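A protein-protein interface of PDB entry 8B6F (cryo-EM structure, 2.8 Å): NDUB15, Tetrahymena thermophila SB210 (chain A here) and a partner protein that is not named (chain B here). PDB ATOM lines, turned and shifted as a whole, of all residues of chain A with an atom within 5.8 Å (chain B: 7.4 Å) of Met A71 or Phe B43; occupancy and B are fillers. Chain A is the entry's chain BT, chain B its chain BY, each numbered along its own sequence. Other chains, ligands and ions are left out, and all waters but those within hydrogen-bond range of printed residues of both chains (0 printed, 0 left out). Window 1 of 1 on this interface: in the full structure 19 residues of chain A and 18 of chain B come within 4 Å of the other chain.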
ATOM      1  N   ARG A   9       1.225   2.384   0.752  1.00  0.00           N
ATOM      2  CA  ARG A   9       1.621   1.442   1.786  1.00  0.00           C
ATOM      3  C   ARG A   9       1.009   0.060   1.600  1.00  0.00           C
ATOM      4  O   ARG A   9       1.336  -0.849   2.371  1.00  0.00           O
ATOM      5  CB  ARG A   9       1.241   1.993   3.168  1.00  0.00           C
ATOM      6  CG  ARG A   9       1.994   1.368   4.328  1.00  0.00           C
ATOM      7  CD  ARG A   9       2.159   2.370   5.461  1.00  0.00           C
ATOM      8  NE  ARG A   9       0.927   3.104   5.725  1.00  0.00           N
ATOM      9  CZ  ARG A   9      -0.010   2.730   6.585  1.00  0.00           C
ATOM     10  NH1 ARG A   9       0.112   1.629   7.308  1.00  0.00           N
ATOM     11  NH2 ARG A   9      -1.099   3.479   6.722  1.00  0.00           N
ATOM     12  N   TYR A  11       1.482  -2.568  -0.780  1.00  0.00           N
ATOM     13  CA  TYR A  11       2.415  -2.856  -1.857  1.00  0.00           C
ATOM     14  C   TYR A  11       1.817  -3.836  -2.860  1.00  0.00           C
ATOM     15  O   TYR A  11       0.922  -4.622  -2.542  1.00  0.00           O
ATOM     16  CB  TYR A  11       3.715  -3.424  -1.290  1.00  0.00           C
ATOM     17  CG  TYR A  11       4.468  -2.454  -0.410  1.00  0.00           C
ATOM     18  CD1 TYR A  11       4.659  -1.136  -0.802  1.00  0.00           C
ATOM     19  CD2 TYR A  11       4.976  -2.853   0.818  1.00  0.00           C
ATOM     20  CE1 TYR A  11       5.343  -0.246  -0.001  1.00  0.00           C
ATOM     21  CE2 TYR A  11       5.662  -1.971   1.627  1.00  0.00           C
ATOM     22  CZ  TYR A  11       5.841  -0.668   1.213  1.00  0.00           C
ATOM     23  OH  TYR A  11       6.522   0.218   2.015  1.00  0.00           O
ATOM     24  N   TYR A  57       8.944 -15.287  -1.549  1.00  0.00           N
ATOM     25  CA  TYR A  57       8.321 -15.162  -0.236  1.00  0.00           C
ATOM     26  C   TYR A  57       9.174 -15.806   0.848  1.00  0.00           C
ATOM     27  O   TYR A  57       9.291 -15.271   1.956  1.00  0.00           O
ATOM     28  CB  TYR A  57       6.923 -15.778  -0.249  1.00  0.00           C
ATOM     29  CG  TYR A  57       6.284 -15.799   1.117  1.00  0.00           C
ATOM     30  CD1 TYR A  57       5.711 -14.657   1.655  1.00  0.00           C
ATOM     31  CD2 TYR A  57       6.254 -16.963   1.871  1.00  0.00           C
ATOM     32  CE1 TYR A  57       5.130 -14.674   2.906  1.00  0.00           C
ATOM     33  CE2 TYR A  57       5.676 -16.991   3.121  1.00  0.00           C
ATOM     34  CZ  TYR A  57       5.113 -15.844   3.632  1.00  0.00           C
ATOM     35  OH  TYR A  57       4.536 -15.872   4.880  1.00  0.00           O
ATOM     36  N   TRP A  60      11.862 -13.326   1.749  1.00  0.00           N
ATOM     37  CA  TRP A  60      11.491 -11.968   2.125  1.00  0.00           C
ATOM     38  C   TRP A  60      11.729 -11.737   3.612  1.00  0.00           C
ATOM     39  O   TRP A  60      11.546 -12.638   4.435  1.00  0.00           O
ATOM     40  CB  TRP A  60      10.025 -11.708   1.780  1.00  0.00           C
ATOM     41  CG  TRP A  60       9.637 -10.275   1.911  1.00  0.00           C
ATOM     42  CD1 TRP A  60       9.652  -9.333   0.929  1.00  0.00           C
ATOM     43  CD2 TRP A  60       9.181  -9.615   3.096  1.00  0.00           C
ATOM     44  NE1 TRP A  60       9.230  -8.125   1.426  1.00  0.00           N
ATOM     45  CE2 TRP A  60       8.935  -8.272   2.755  1.00  0.00           C
ATOM     46  CE3 TRP A  60       8.954 -10.030   4.412  1.00  0.00           C
ATOM     47  CZ2 TRP A  60       8.475  -7.340   3.679  1.00  0.00           C
ATOM     48  CZ3 TRP A  60       8.497  -9.102   5.329  1.00  0.00           C
ATOM     49  CH2 TRP A  60       8.261  -7.772   4.957  1.00  0.00           C
ATOM     50  N   TYR A  62      12.102  -8.345   6.842  1.00  0.00           N
ATOM     51  CA  TYR A  62      11.881  -6.959   7.234  1.00  0.00           C
ATOM     52  C   TYR A  62      13.196  -6.189   7.237  1.00  0.00           C
ATOM     53  O   TYR A  62      14.203  -6.664   7.770  1.00  0.00           O
ATOM     54  CB  TYR A  62      11.234  -6.891   8.616  1.00  0.00           C
ATOM     55  CG  TYR A  62       9.767  -7.251   8.631  1.00  0.00           C
ATOM     56  CD1 TYR A  62       8.818  -6.398   8.084  1.00  0.00           C
ATOM     57  CD2 TYR A  62       9.331  -8.434   9.210  1.00  0.00           C
ATOM     58  CE1 TYR A  62       7.476  -6.720   8.101  1.00  0.00           C
ATOM     59  CE2 TYR A  62       7.992  -8.763   9.232  1.00  0.00           C
ATOM     60  CZ  TYR A  62       7.071  -7.903   8.677  1.00  0.00           C
ATOM     61  OH  TYR A  62       5.736  -8.228   8.700  1.00  0.00           O
ATOM     62  N   GLY A  66      10.528  -2.691  13.633  1.00  0.00           N
ATOM     63  CA  GLY A  66       9.224  -2.077  13.735  1.00  0.00           C
ATOM     64  C   GLY A  66       8.497  -1.886  12.424  1.00  0.00           C
ATOM     65  O   GLY A  66       7.395  -1.324  12.424  1.00  0.00           O
ATOM     66  N   GLN A  67       9.070  -2.333  11.306  1.00  0.00           N
ATOM     67  CA  GLN A  67       8.408  -2.165  10.020  1.00  0.00           C
ATOM     68  C   GLN A  67       7.108  -2.950   9.948  1.00  0.00           C
ATOM     69  O   GLN A  67       6.220  -2.592   9.167  1.00  0.00           O
ATOM     70  CB  GLN A  67       9.343  -2.594   8.888  1.00  0.00           C
ATOM     71  CG  GLN A  67       8.791  -2.326   7.498  1.00  0.00           C
ATOM     72  CD  GLN A  67       9.725  -2.792   6.404  1.00  0.00           C
ATOM     73  OE1 GLN A  67      10.623  -3.595   6.642  1.00  0.00           O
ATOM     74  NE2 GLN A  67       9.520  -2.285   5.194  1.00  0.00           N
ATOM     75  N   TRP A  68       6.980  -4.016  10.741  1.00  0.00           N
ATOM     76  CA  TRP A  68       5.800  -4.871  10.655  1.00  0.00           C
ATOM     77  C   TRP A  68       4.532  -4.111  11.019  1.00  0.00           C
ATOM     78  O   TRP A  68       3.500  -4.263  10.356  1.00  0.00           O
ATOM     79  CB  TRP A  68       5.967  -6.102  11.549  1.00  0.00           C
ATOM     80  CG  TRP A  68       6.608  -5.839  12.877  1.00  0.00           C
ATOM     81  CD1 TRP A  68       5.987  -5.455  14.024  1.00  0.00           C
ATOM     82  CD2 TRP A  68       8.001  -5.952  13.191  1.00  0.00           C
ATOM     83  NE1 TRP A  68       6.906  -5.319  15.036  1.00  0.00           N
ATOM     84  CE2 TRP A  68       8.150  -5.617  14.550  1.00  0.00           C
ATOM     85  CE3 TRP A  68       9.136  -6.302  12.454  1.00  0.00           C
ATOM     86  CZ2 TRP A  68       9.388  -5.622  15.188  1.00  0.00           C
ATOM     87  CZ3 TRP A  68      10.366  -6.306  13.088  1.00  0.00           C
ATOM     88  CH2 TRP A  68      10.482  -5.969  14.443  1.00  0.00           C
ATOM     89  N   TRP A  69       4.585  -3.288  12.067  1.00  0.00           N
ATOM     90  CA  TRP A  69       3.395  -2.552  12.480  1.00  0.00           C
ATOM     91  C   TRP A  69       2.907  -1.625  11.374  1.00  0.00           C
ATOM     92  O   TRP A  69       1.705  -1.557  11.096  1.00  0.00           O
ATOM     93  CB  TRP A  69       3.682  -1.752  13.752  1.00  0.00           C
ATOM     94  CG  TRP A  69       3.945  -2.599  14.954  1.00  0.00           C
ATOM     95  CD1 TRP A  69       5.122  -2.714  15.632  1.00  0.00           C
ATOM     96  CD2 TRP A  69       3.011  -3.452  15.624  1.00  0.00           C
ATOM     97  NE1 TRP A  69       4.977  -3.587  16.683  1.00  0.00           N
ATOM     98  CE2 TRP A  69       3.689  -4.051  16.701  1.00  0.00           C
ATOM     99  CE3 TRP A  69       1.663  -3.765  15.417  1.00  0.00           C
ATOM    100  CZ2 TRP A  69       3.069  -4.947  17.568  1.00  0.00           C
ATOM    101  CZ3 TRP A  69       1.049  -4.652  16.278  1.00  0.00           C
ATOM    102  CH2 TRP A  69       1.752  -5.234  17.342  1.00  0.00           C
ATOM    103  N   SER A  70       3.825  -0.905  10.729  1.00  0.00           N
ATOM    104  CA  SER A  70       3.437   0.084   9.730  1.00  0.00           C
ATOM    105  C   SER A  70       3.004  -0.571   8.423  1.00  0.00           C
ATOM    106  O   SER A  70       2.071  -0.094   7.770  1.00  0.00           O
ATOM    107  CB  SER A  70       4.595   1.050   9.470  1.00  0.00           C
ATOM    108  OG  SER A  70       5.003   1.696  10.663  1.00  0.00           O
ATOM    109  N   MET A  71       3.664  -1.657   8.029  1.00  0.00           N
ATOM    110  CA  MET A  71       3.378  -2.275   6.741  1.00  0.00           C
ATOM    111  C   MET A  71       1.919  -2.703   6.668  1.00  0.00           C
ATOM    112  O   MET A  71       1.359  -3.235   7.629  1.00  0.00           O
ATOM    113  CB  MET A  71       4.291  -3.481   6.517  1.00  0.00           C
ATOM    114  CG  MET A  71       4.868  -3.557   5.113  1.00  0.00           C
ATOM    115  SD  MET A  71       5.693  -5.124   4.776  1.00  0.00           S
ATOM    116  CE  MET A  71       4.288  -6.231   4.684  1.00  0.00           C
ATOM    117  N   GLY A  72       1.303  -2.472   5.512  1.00  0.00           N
ATOM    118  CA  GLY A  72      -0.098  -2.784   5.327  1.00  0.00           C
ATOM    119  C   GLY A  72      -1.003  -1.730   5.929  1.00  0.00           C
ATOM    120  O   GLY A  72      -1.038  -0.591   5.455  1.00  0.00           O
ATOM    121  N   SER A  73      -1.749  -2.096   6.968  1.00  0.00           N
ATOM    122  CA  SER A  73      -2.589  -1.158   7.697  1.00  0.00           C
ATOM    123  C   SER A  73      -2.378  -1.362   9.189  1.00  0.00           C
ATOM    124  O   SER A  73      -2.457  -2.491   9.682  1.00  0.00           O
ATOM    125  CB  SER A  73      -4.068  -1.329   7.336  1.00  0.00           C
ATOM    126  OG  SER A  73      -4.493  -2.662   7.539  1.00  0.00           O
ATOM    127  N   LEU A  74      -2.111  -0.266   9.901  1.00  0.00           N
ATOM    128  CA  LEU A  74      -1.818  -0.361  11.327  1.00  0.00           C
ATOM    129  C   LEU A  74      -3.006  -0.915  12.100  1.00  0.00           C
ATOM    130  O   LEU A  74      -2.837  -1.748  12.998  1.00  0.00           O
ATOM    131  CB  LEU A  74      -1.419   1.013  11.865  1.00  0.00           C
ATOM    132  CG  LEU A  74      -1.067   1.097  13.352  1.00  0.00           C
ATOM    133  CD1 LEU A  74       0.108   0.197  13.688  1.00  0.00           C
ATOM    134  CD2 LEU A  74      -0.766   2.531  13.738  1.00  0.00           C
ATOM    135  N   ASN A  77      -3.323  -4.657  11.475  1.00  0.00           N
ATOM    136  CA  ASN A  77      -2.220  -5.354  12.126  1.00  0.00           C
ATOM    137  C   ASN A  77      -2.443  -5.449  13.629  1.00  0.00           C
ATOM    138  O   ASN A  77      -2.210  -6.502  14.233  1.00  0.00           O
ATOM    139  CB  ASN A  77      -0.901  -4.643  11.826  1.00  0.00           C
ATOM    140  CG  ASN A  77      -0.485  -4.774  10.376  1.00  0.00           C
ATOM    141  OD1 ASN A  77      -0.740  -5.791   9.735  1.00  0.00           O
ATOM    142  ND2 ASN A  77       0.165  -3.743   9.853  1.00  0.00           N
ATOM    143  N   ARG B  34      -7.110  -7.955   0.316  1.00  0.00           N
ATOM    144  CA  ARG B  34      -5.728  -7.496   0.378  1.00  0.00           C
ATOM    145  C   ARG B  34      -5.282  -7.261   1.813  1.00  0.00           C
ATOM    146  O   ARG B  34      -4.166  -7.634   2.192  1.00  0.00           O
ATOM    147  CB  ARG B  34      -5.563  -6.221  -0.445  1.00  0.00           C
ATOM    148  CG  ARG B  34      -5.839  -6.405  -1.927  1.00  0.00           C
ATOM    149  CD  ARG B  34      -5.280  -5.251  -2.734  1.00  0.00           C
ATOM    150  NE  ARG B  34      -3.828  -5.317  -2.811  1.00  0.00           N
ATOM    151  CZ  ARG B  34      -3.153  -5.989  -3.733  1.00  0.00           C
ATOM    152  NH1 ARG B  34      -3.768  -6.635  -4.709  1.00  0.00           N
ATOM    153  NH2 ARG B  34      -1.827  -6.020  -3.668  1.00  0.00           N
ATOM    154  N   ILE B  36      -6.588  -8.448   4.733  1.00  0.00           N
ATOM    155  CA  ILE B  36      -6.710  -9.537   5.695  1.00  0.00           C
ATOM    156  C   ILE B  36      -5.902 -10.755   5.267  1.00  0.00           C
ATOM    157  O   ILE B  36      -5.256 -11.396   6.099  1.00  0.00           O
ATOM    158  CB  ILE B  36      -8.198  -9.890   5.896  1.00  0.00           C
ATOM    159  CG1 ILE B  36      -8.986  -8.667   6.383  1.00  0.00           C
ATOM    160  CG2 ILE B  36      -8.354 -11.049   6.875  1.00  0.00           C
ATOM    161  CD1 ILE B  36      -8.508  -8.089   7.703  1.00  0.00           C
ATOM    162  N   PHE B  37      -5.926 -11.102   3.981  1.00  0.00           N
ATOM    163  CA  PHE B  37      -5.314 -12.343   3.529  1.00  0.00           C
ATOM    164  C   PHE B  37      -3.833 -12.215   3.202  1.00  0.00           C
ATOM    165  O   PHE B  37      -3.169 -13.244   3.046  1.00  0.00           O
ATOM    166  CB  PHE B  37      -6.046 -12.877   2.291  1.00  0.00           C
ATOM    167  CG  PHE B  37      -7.453 -13.349   2.561  1.00  0.00           C
ATOM    168  CD1 PHE B  37      -7.871 -13.670   3.842  1.00  0.00           C
ATOM    169  CD2 PHE B  37      -8.353 -13.482   1.518  1.00  0.00           C
ATOM    170  CE1 PHE B  37      -9.157 -14.108   4.074  1.00  0.00           C
ATOM    171  CE2 PHE B  37      -9.641 -13.919   1.746  1.00  0.00           C
ATOM    172  CZ  PHE B  37     -10.043 -14.232   3.024  1.00  0.00           C
ATOM    173  N   ILE B  38      -3.296 -11.000   3.098  1.00  0.00           N
ATOM    174  CA  ILE B  38      -1.907 -10.832   2.681  1.00  0.00           C
ATOM    175  C   ILE B  38      -1.118 -10.050   3.723  1.00  0.00           C
ATOM    176  O   ILE B  38      -0.169 -10.569   4.317  1.00  0.00           O
ATOM    177  CB  ILE B  38      -1.825 -10.139   1.309  1.00  0.00           C
ATOM    178  CG1 ILE B  38      -2.685 -10.888   0.288  1.00  0.00           C
ATOM    179  CG2 ILE B  38      -0.377 -10.068   0.841  1.00  0.00           C
ATOM    180  CD1 ILE B  38      -2.761 -10.221  -1.065  1.00  0.00           C
ATOM    181  N   TYR B  39      -1.509  -8.797   3.952  1.00  0.00           N
ATOM    182  CA  TYR B  39      -0.701  -7.917   4.790  1.00  0.00           C
ATOM    183  C   TYR B  39      -0.792  -8.305   6.257  1.00  0.00           C
ATOM    184  O   TYR B  39       0.223  -8.329   6.963  1.00  0.00           O
ATOM    185  CB  TYR B  39      -1.137  -6.467   4.595  1.00  0.00           C
ATOM    186  CG  TYR B  39      -1.187  -6.041   3.148  1.00  0.00           C
ATOM    187  CD1 TYR B  39      -0.310  -6.578   2.215  1.00  0.00           C
ATOM    188  CD2 TYR B  39      -2.117  -5.112   2.713  1.00  0.00           C
ATOM    189  CE1 TYR B  39      -0.356  -6.196   0.893  1.00  0.00           C
ATOM    190  CE2 TYR B  39      -2.171  -4.723   1.391  1.00  0.00           C
ATOM    191  CZ  TYR B  39      -1.288  -5.269   0.487  1.00  0.00           C
ATOM    192  OH  TYR B  39      -1.337  -4.885  -0.832  1.00  0.00           O
ATOM    193  N   SER B  40      -1.993  -8.610   6.732  1.00  0.00           N
ATOM    194  CA  SER B  40      -2.208  -8.899   8.142  1.00  0.00           C
ATOM    195  C   SER B  40      -1.962 -10.362   8.478  1.00  0.00           C
ATOM    196  O   SER B  40      -1.410 -10.669   9.540  1.00  0.00           O
ATOM    197  CB  SER B  40      -3.633  -8.512   8.537  1.00  0.00           C
ATOM    198  OG  SER B  40      -3.836  -8.682   9.926  1.00  0.00           O
ATOM    199  N   SER B  41      -2.361 -11.275   7.597  1.00  0.00           N
ATOM    200  CA  SER B  41      -2.253 -12.702   7.878  1.00  0.00           C
ATOM    201  C   SER B  41      -0.894 -13.268   7.478  1.00  0.00           C
ATOM    202  O   SER B  41      -0.203 -13.877   8.300  1.00  0.00           O
ATOM    203  CB  SER B  41      -3.372 -13.456   7.158  1.00  0.00           C
ATOM    204  OG  SER B  41      -3.288 -14.836   7.447  1.00  0.00           O
ATOM    205  N   ILE B  42      -0.500 -13.080   6.221  1.00  0.00           N
ATOM    206  CA  ILE B  42       0.750 -13.661   5.743  1.00  0.00           C
ATOM    207  C   ILE B  42       1.942 -12.910   6.323  1.00  0.00           C
ATOM    208  O   ILE B  42       2.769 -13.482   7.039  1.00  0.00           O
ATOM    209  CB  ILE B  42       0.782 -13.677   4.204  1.00  0.00           C
ATOM    210  CG1 ILE B  42      -0.317 -14.590   3.653  1.00  0.00           C
ATOM    211  CG2 ILE B  42       2.145 -14.108   3.694  1.00  0.00           C
ATOM    212  CD1 ILE B  42      -0.136 -16.062   3.971  1.00  0.00           C
ATOM    213  N   PHE B  43       2.045 -11.615   6.034  1.00  0.00           N
ATOM    214  CA  PHE B  43       3.239 -10.878   6.430  1.00  0.00           C
ATOM    215  C   PHE B  43       3.242 -10.595   7.927  1.00  0.00           C
ATOM    216  O   PHE B  43       4.124 -11.061   8.656  1.00  0.00           O
ATOM    217  CB  PHE B  43       3.348  -9.589   5.619  1.00  0.00           C
ATOM    218  CG  PHE B  43       3.653  -9.826   4.171  1.00  0.00           C
ATOM    219  CD1 PHE B  43       4.942 -10.123   3.766  1.00  0.00           C
ATOM    220  CD2 PHE B  43       2.653  -9.768   3.219  1.00  0.00           C
ATOM    221  CE1 PHE B  43       5.229 -10.350   2.437  1.00  0.00           C
ATOM    222  CE2 PHE B  43       2.934  -9.994   1.888  1.00  0.00           C
ATOM    223  CZ  PHE B  43       4.225 -10.286   1.497  1.00  0.00           C
ATOM    224  N   PHE B  44       2.258  -9.845   8.417  1.00  0.00           N
ATOM    225  CA  PHE B  44       2.238  -9.550   9.846  1.00  0.00           C
ATOM    226  C   PHE B  44       2.072 -10.825  10.661  1.00  0.00           C
ATOM    227  O   PHE B  44       2.706 -10.986  11.709  1.00  0.00           O
ATOM    228  CB  PHE B  44       1.133  -8.556  10.184  1.00  0.00           C
ATOM    229  CG  PHE B  44       1.138  -8.129  11.623  1.00  0.00           C
ATOM    230  CD1 PHE B  44       1.968  -7.109  12.054  1.00  0.00           C
ATOM    231  CD2 PHE B  44       0.325  -8.761  12.548  1.00  0.00           C
ATOM    232  CE1 PHE B  44       1.981  -6.721  13.374  1.00  0.00           C
ATOM    233  CE2 PHE B  44       0.333  -8.379  13.872  1.00  0.00           C
ATOM    234  CZ  PHE B  44       1.162  -7.357  14.286  1.00  0.00           C
ATOM    235  N   GLY B  45       1.224 -11.736  10.204  1.00  0.00           N
ATOM    236  CA  GLY B  45       1.014 -12.977  10.917  1.00  0.00           C
ATOM    237  C   GLY B  45       2.160 -13.956  10.773  1.00  0.00           C
ATOM    238  O   GLY B  45       2.836 -14.267  11.757  1.00  0.00           O
ATOM    239  N   GLU B  46       2.398 -14.457   9.560  1.00  0.00           N
ATOM    240  CA  GLU B  46       3.396 -15.508   9.390  1.00  0.00           C
ATOM    241  C   GLU B  46       4.817 -14.965   9.517  1.00  0.00           C
ATOM    242  O   GLU B  46       5.656 -15.561  10.199  1.00  0.00           O
ATOM    243  CB  GLU B  46       3.204 -16.210   8.045  1.00  0.00           C
ATOM    244  CG  GLU B  46       4.095 -17.426   7.847  1.00  0.00           C
ATOM    245  CD  GLU B  46       3.882 -18.492   8.906  1.00  0.00           C
ATOM    246  OE1 GLU B  46       2.825 -18.476   9.568  1.00  0.00           O
ATOM    247  OE2 GLU B  46       4.775 -19.347   9.077  1.00  0.00           O
ATOM    248  N   LYS B  47       5.111 -13.834   8.874  1.00  0.00           N
ATOM    249  CA  LYS B  47       6.488 -13.347   8.898  1.00  0.00           C
ATOM    250  C   LYS B  47       6.853 -12.727  10.242  1.00  0.00           C
ATOM    251  O   LYS B  47       7.958 -12.957  10.743  1.00  0.00           O
ATOM    252  CB  LYS B  47       6.723 -12.347   7.762  1.00  0.00           C
ATOM    253  CG  LYS B  47       6.893 -12.993   6.391  1.00  0.00           C
ATOM    254  CD  LYS B  47       8.190 -13.782   6.288  1.00  0.00           C
ATOM    255  CE  LYS B  47       8.346 -14.404   4.912  1.00  0.00           C
ATOM    256  NZ  LYS B  47       9.584 -15.221   4.810  1.00  0.00           N
ATOM    257  N   PHE B  48       5.970 -11.925  10.838  1.00  0.00           N
ATOM    258  CA  PHE B  48       6.315 -11.275  12.100  1.00  0.00           C
ATOM    259  C   PHE B  48       5.906 -12.104  13.315  1.00  0.00           C
ATOM    260  O   PHE B  48       6.756 -12.490  14.123  1.00  0.00           O
ATOM    261  CB  PHE B  48       5.673  -9.885  12.179  1.00  0.00           C
ATOM    262  CG  PHE B  48       5.627  -9.326  13.573  1.00  0.00           C
ATOM    263  CD1 PHE B  48       6.787  -8.934  14.216  1.00  0.00           C
ATOM    264  CD2 PHE B  48       4.421  -9.185  14.238  1.00  0.00           C
ATOM    265  CE1 PHE B  48       6.747  -8.419  15.500  1.00  0.00           C
ATOM    266  CE2 PHE B  48       4.374  -8.670  15.520  1.00  0.00           C
ATOM    267  CZ  PHE B  48       5.538  -8.287  16.151  1.00  0.00           C
ATOM    268  N   MET B  49       4.611 -12.389  13.460  1.00  0.00           N
ATOM    269  CA  MET B  49       4.145 -13.038  14.682  1.00  0.00           C
ATOM    270  C   MET B  49       4.733 -14.436  14.839  1.00  0.00           C
ATOM    271  O   MET B  49       5.094 -14.841  15.949  1.00  0.00           O
ATOM    272  CB  MET B  49       2.618 -13.097  14.702  1.00  0.00           C
ATOM    273  CG  MET B  49       1.955 -11.745  14.907  1.00  0.00           C
ATOM    274  SD  MET B  49       0.159 -11.839  15.036  1.00  0.00           S
ATOM    275  CE  MET B  49      -0.039 -12.773  16.550  1.00  0.00           C
ATOM    276  N   ILE B  50       4.835 -15.188  13.745  1.00  0.00           N
ATOM    277  CA  ILE B  50       5.313 -16.565  13.808  1.00  0.00           C
ATOM    278  C   ILE B  50       6.821 -16.616  13.624  1.00  0.00           C
ATOM    279  O   ILE B  50       7.550 -17.086  14.504  1.00  0.00           O
ATOM    280  CB  ILE B  50       4.612 -17.441  12.752  1.00  0.00           C
ATOM    281  CG1 ILE B  50       3.121 -17.587  13.059  1.00  0.00           C
ATOM    282  CG2 ILE B  50       5.263 -18.822  12.665  1.00  0.00           C
ATOM    283  CD1 ILE B  50       2.810 -18.237  14.381  1.00  0.00           C
ATOM    284  N   GLU B  51       7.298 -16.142  12.474  1.00  0.00           N
ATOM    285  CA  GLU B  51       8.705 -16.328  12.139  1.00  0.00           C
ATOM    286  C   GLU B  51       9.606 -15.416  12.960  1.00  0.00           C
ATOM    287  O   GLU B  51      10.669 -15.845  13.421  1.00  0.00           O
ATOM    288  CB  GLU B  51       8.922 -16.090  10.645  1.00  0.00           C
ATOM    289  CG  GLU B  51      10.381 -16.115  10.225  1.00  0.00           C
ATOM    290  CD  GLU B  51      10.556 -15.997   8.728  1.00  0.00           C
ATOM    291  OE1 GLU B  51       9.582 -16.270   7.994  1.00  0.00           O
ATOM    292  OE2 GLU B  51      11.661 -15.627   8.283  1.00  0.00           O
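Of the 17 printed residues of chain B, 9 touch a printed residue of chain A.
Printed residues of chain B that touch a printed residue of chain A: Arg B34, Tyr B39, Ser B40, Ile B42, Phe B43, Phe B44, Glu B46, Lys B47 and Phe B48.
Of the 15 printed residues of chain A, 9 touch a printed residue of chain B.
Hydrophobic or aromatic side chains of chain A within 4 Å of the printed part of chain B: Tyr A57, Tyr A62, Trp A68, Trp A69 and Met A71.
NH1 of Arg A9 sits at hydrogen-bond distance from O of Gly A72.
The backbone NH (N) of Met B49 is in hydrogen-bond range of the backbone carbonyl oxygen (O) of Phe B44 (2.9 Å).
The backbone carbonyl oxygen of Phe B43 is in hydrogen-bond range of the backbone NH of Phe B48 (3.0 Å).
NZ of Lys B47 lies within salt-bridge range of OE1 of Glu B51 (3.4 Å).
The backbone carbonyl oxygen (O) of Trp A68 lies within hydrogen-bond range of the side-chain amide nitrogen (ND2) of Asn A77, 3.4 Å away.
The backbone carbonyl oxygen of Ser B40 is in hydrogen-bond range of the backbone NH of Gly B45, 2.9 Å away.
Tyr A57 touches Ile B42 (CE1 to CG2, 3.1 Å).
Glu B46 touches Tyr A57.
Trp A68 touches Phe B44 (O to CD1, 3.7 Å).
Trp A68 touches Phe B48 (NE1 to CE1, 3.1 Å).
Phe B44 touches Trp A69 (CZ to CZ3, 3.4 Å).
Phe B43 touches Met A71 (CB to CE, 3.6 Å).
Gly A72 touches Tyr B39 (CA to CB, 3.9 Å).
Tyr B39 touches Asn A77.
CA of Ser B40 touches OD1 of Asn A77, 3.8 Å away.
Phe B44 touches Asn A77 (CE2 to O, 3.2 Å).
Printed residues of chain B within 4 Å of Tyr A57: Ile B42, Glu B46 and Lys B47.
Of chain B, only Phe B43 (3.6 Å) comes within 4 Å of Met A71.
Of the printed residues of chain A, Phe B44 touches Tyr A62 (3.8 Å), Trp A68 (3.7 Å), Trp A69 (3.4 Å) and Asn A77 (3.2 Å).
Met B49 touches none of the printed residues of chain A.
The nearest residue of chain B that does not touch Met A71 is Tyr B39 (5.1 Å).
The nearest printed residue of chain A that does not touch Phe B43 is Trp A60 (4.02 Å).
NZ of Lys B47 lies within hydrogen-bond range of O of Tyr A57, 2.9 Å away.
The backbone carbonyl oxygen (O) of Trp A60 sits at hydrogen-bond distance from the side-chain amino group (NZ) of Lys B47 (3.3 Å).
The backbone carbonyl oxygen (O) of Tyr A11 is in hydrogen-bond range of the guanidinium group (NH2) of Arg B34, 3.3 Å away.
O of Tyr A11 lies within hydrogen-bond range of OH of Tyr B39, at 2.8 Å.
O of Phe B43 lies within hydrogen-bond range of OH of Tyr A62 (3.3 Å).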
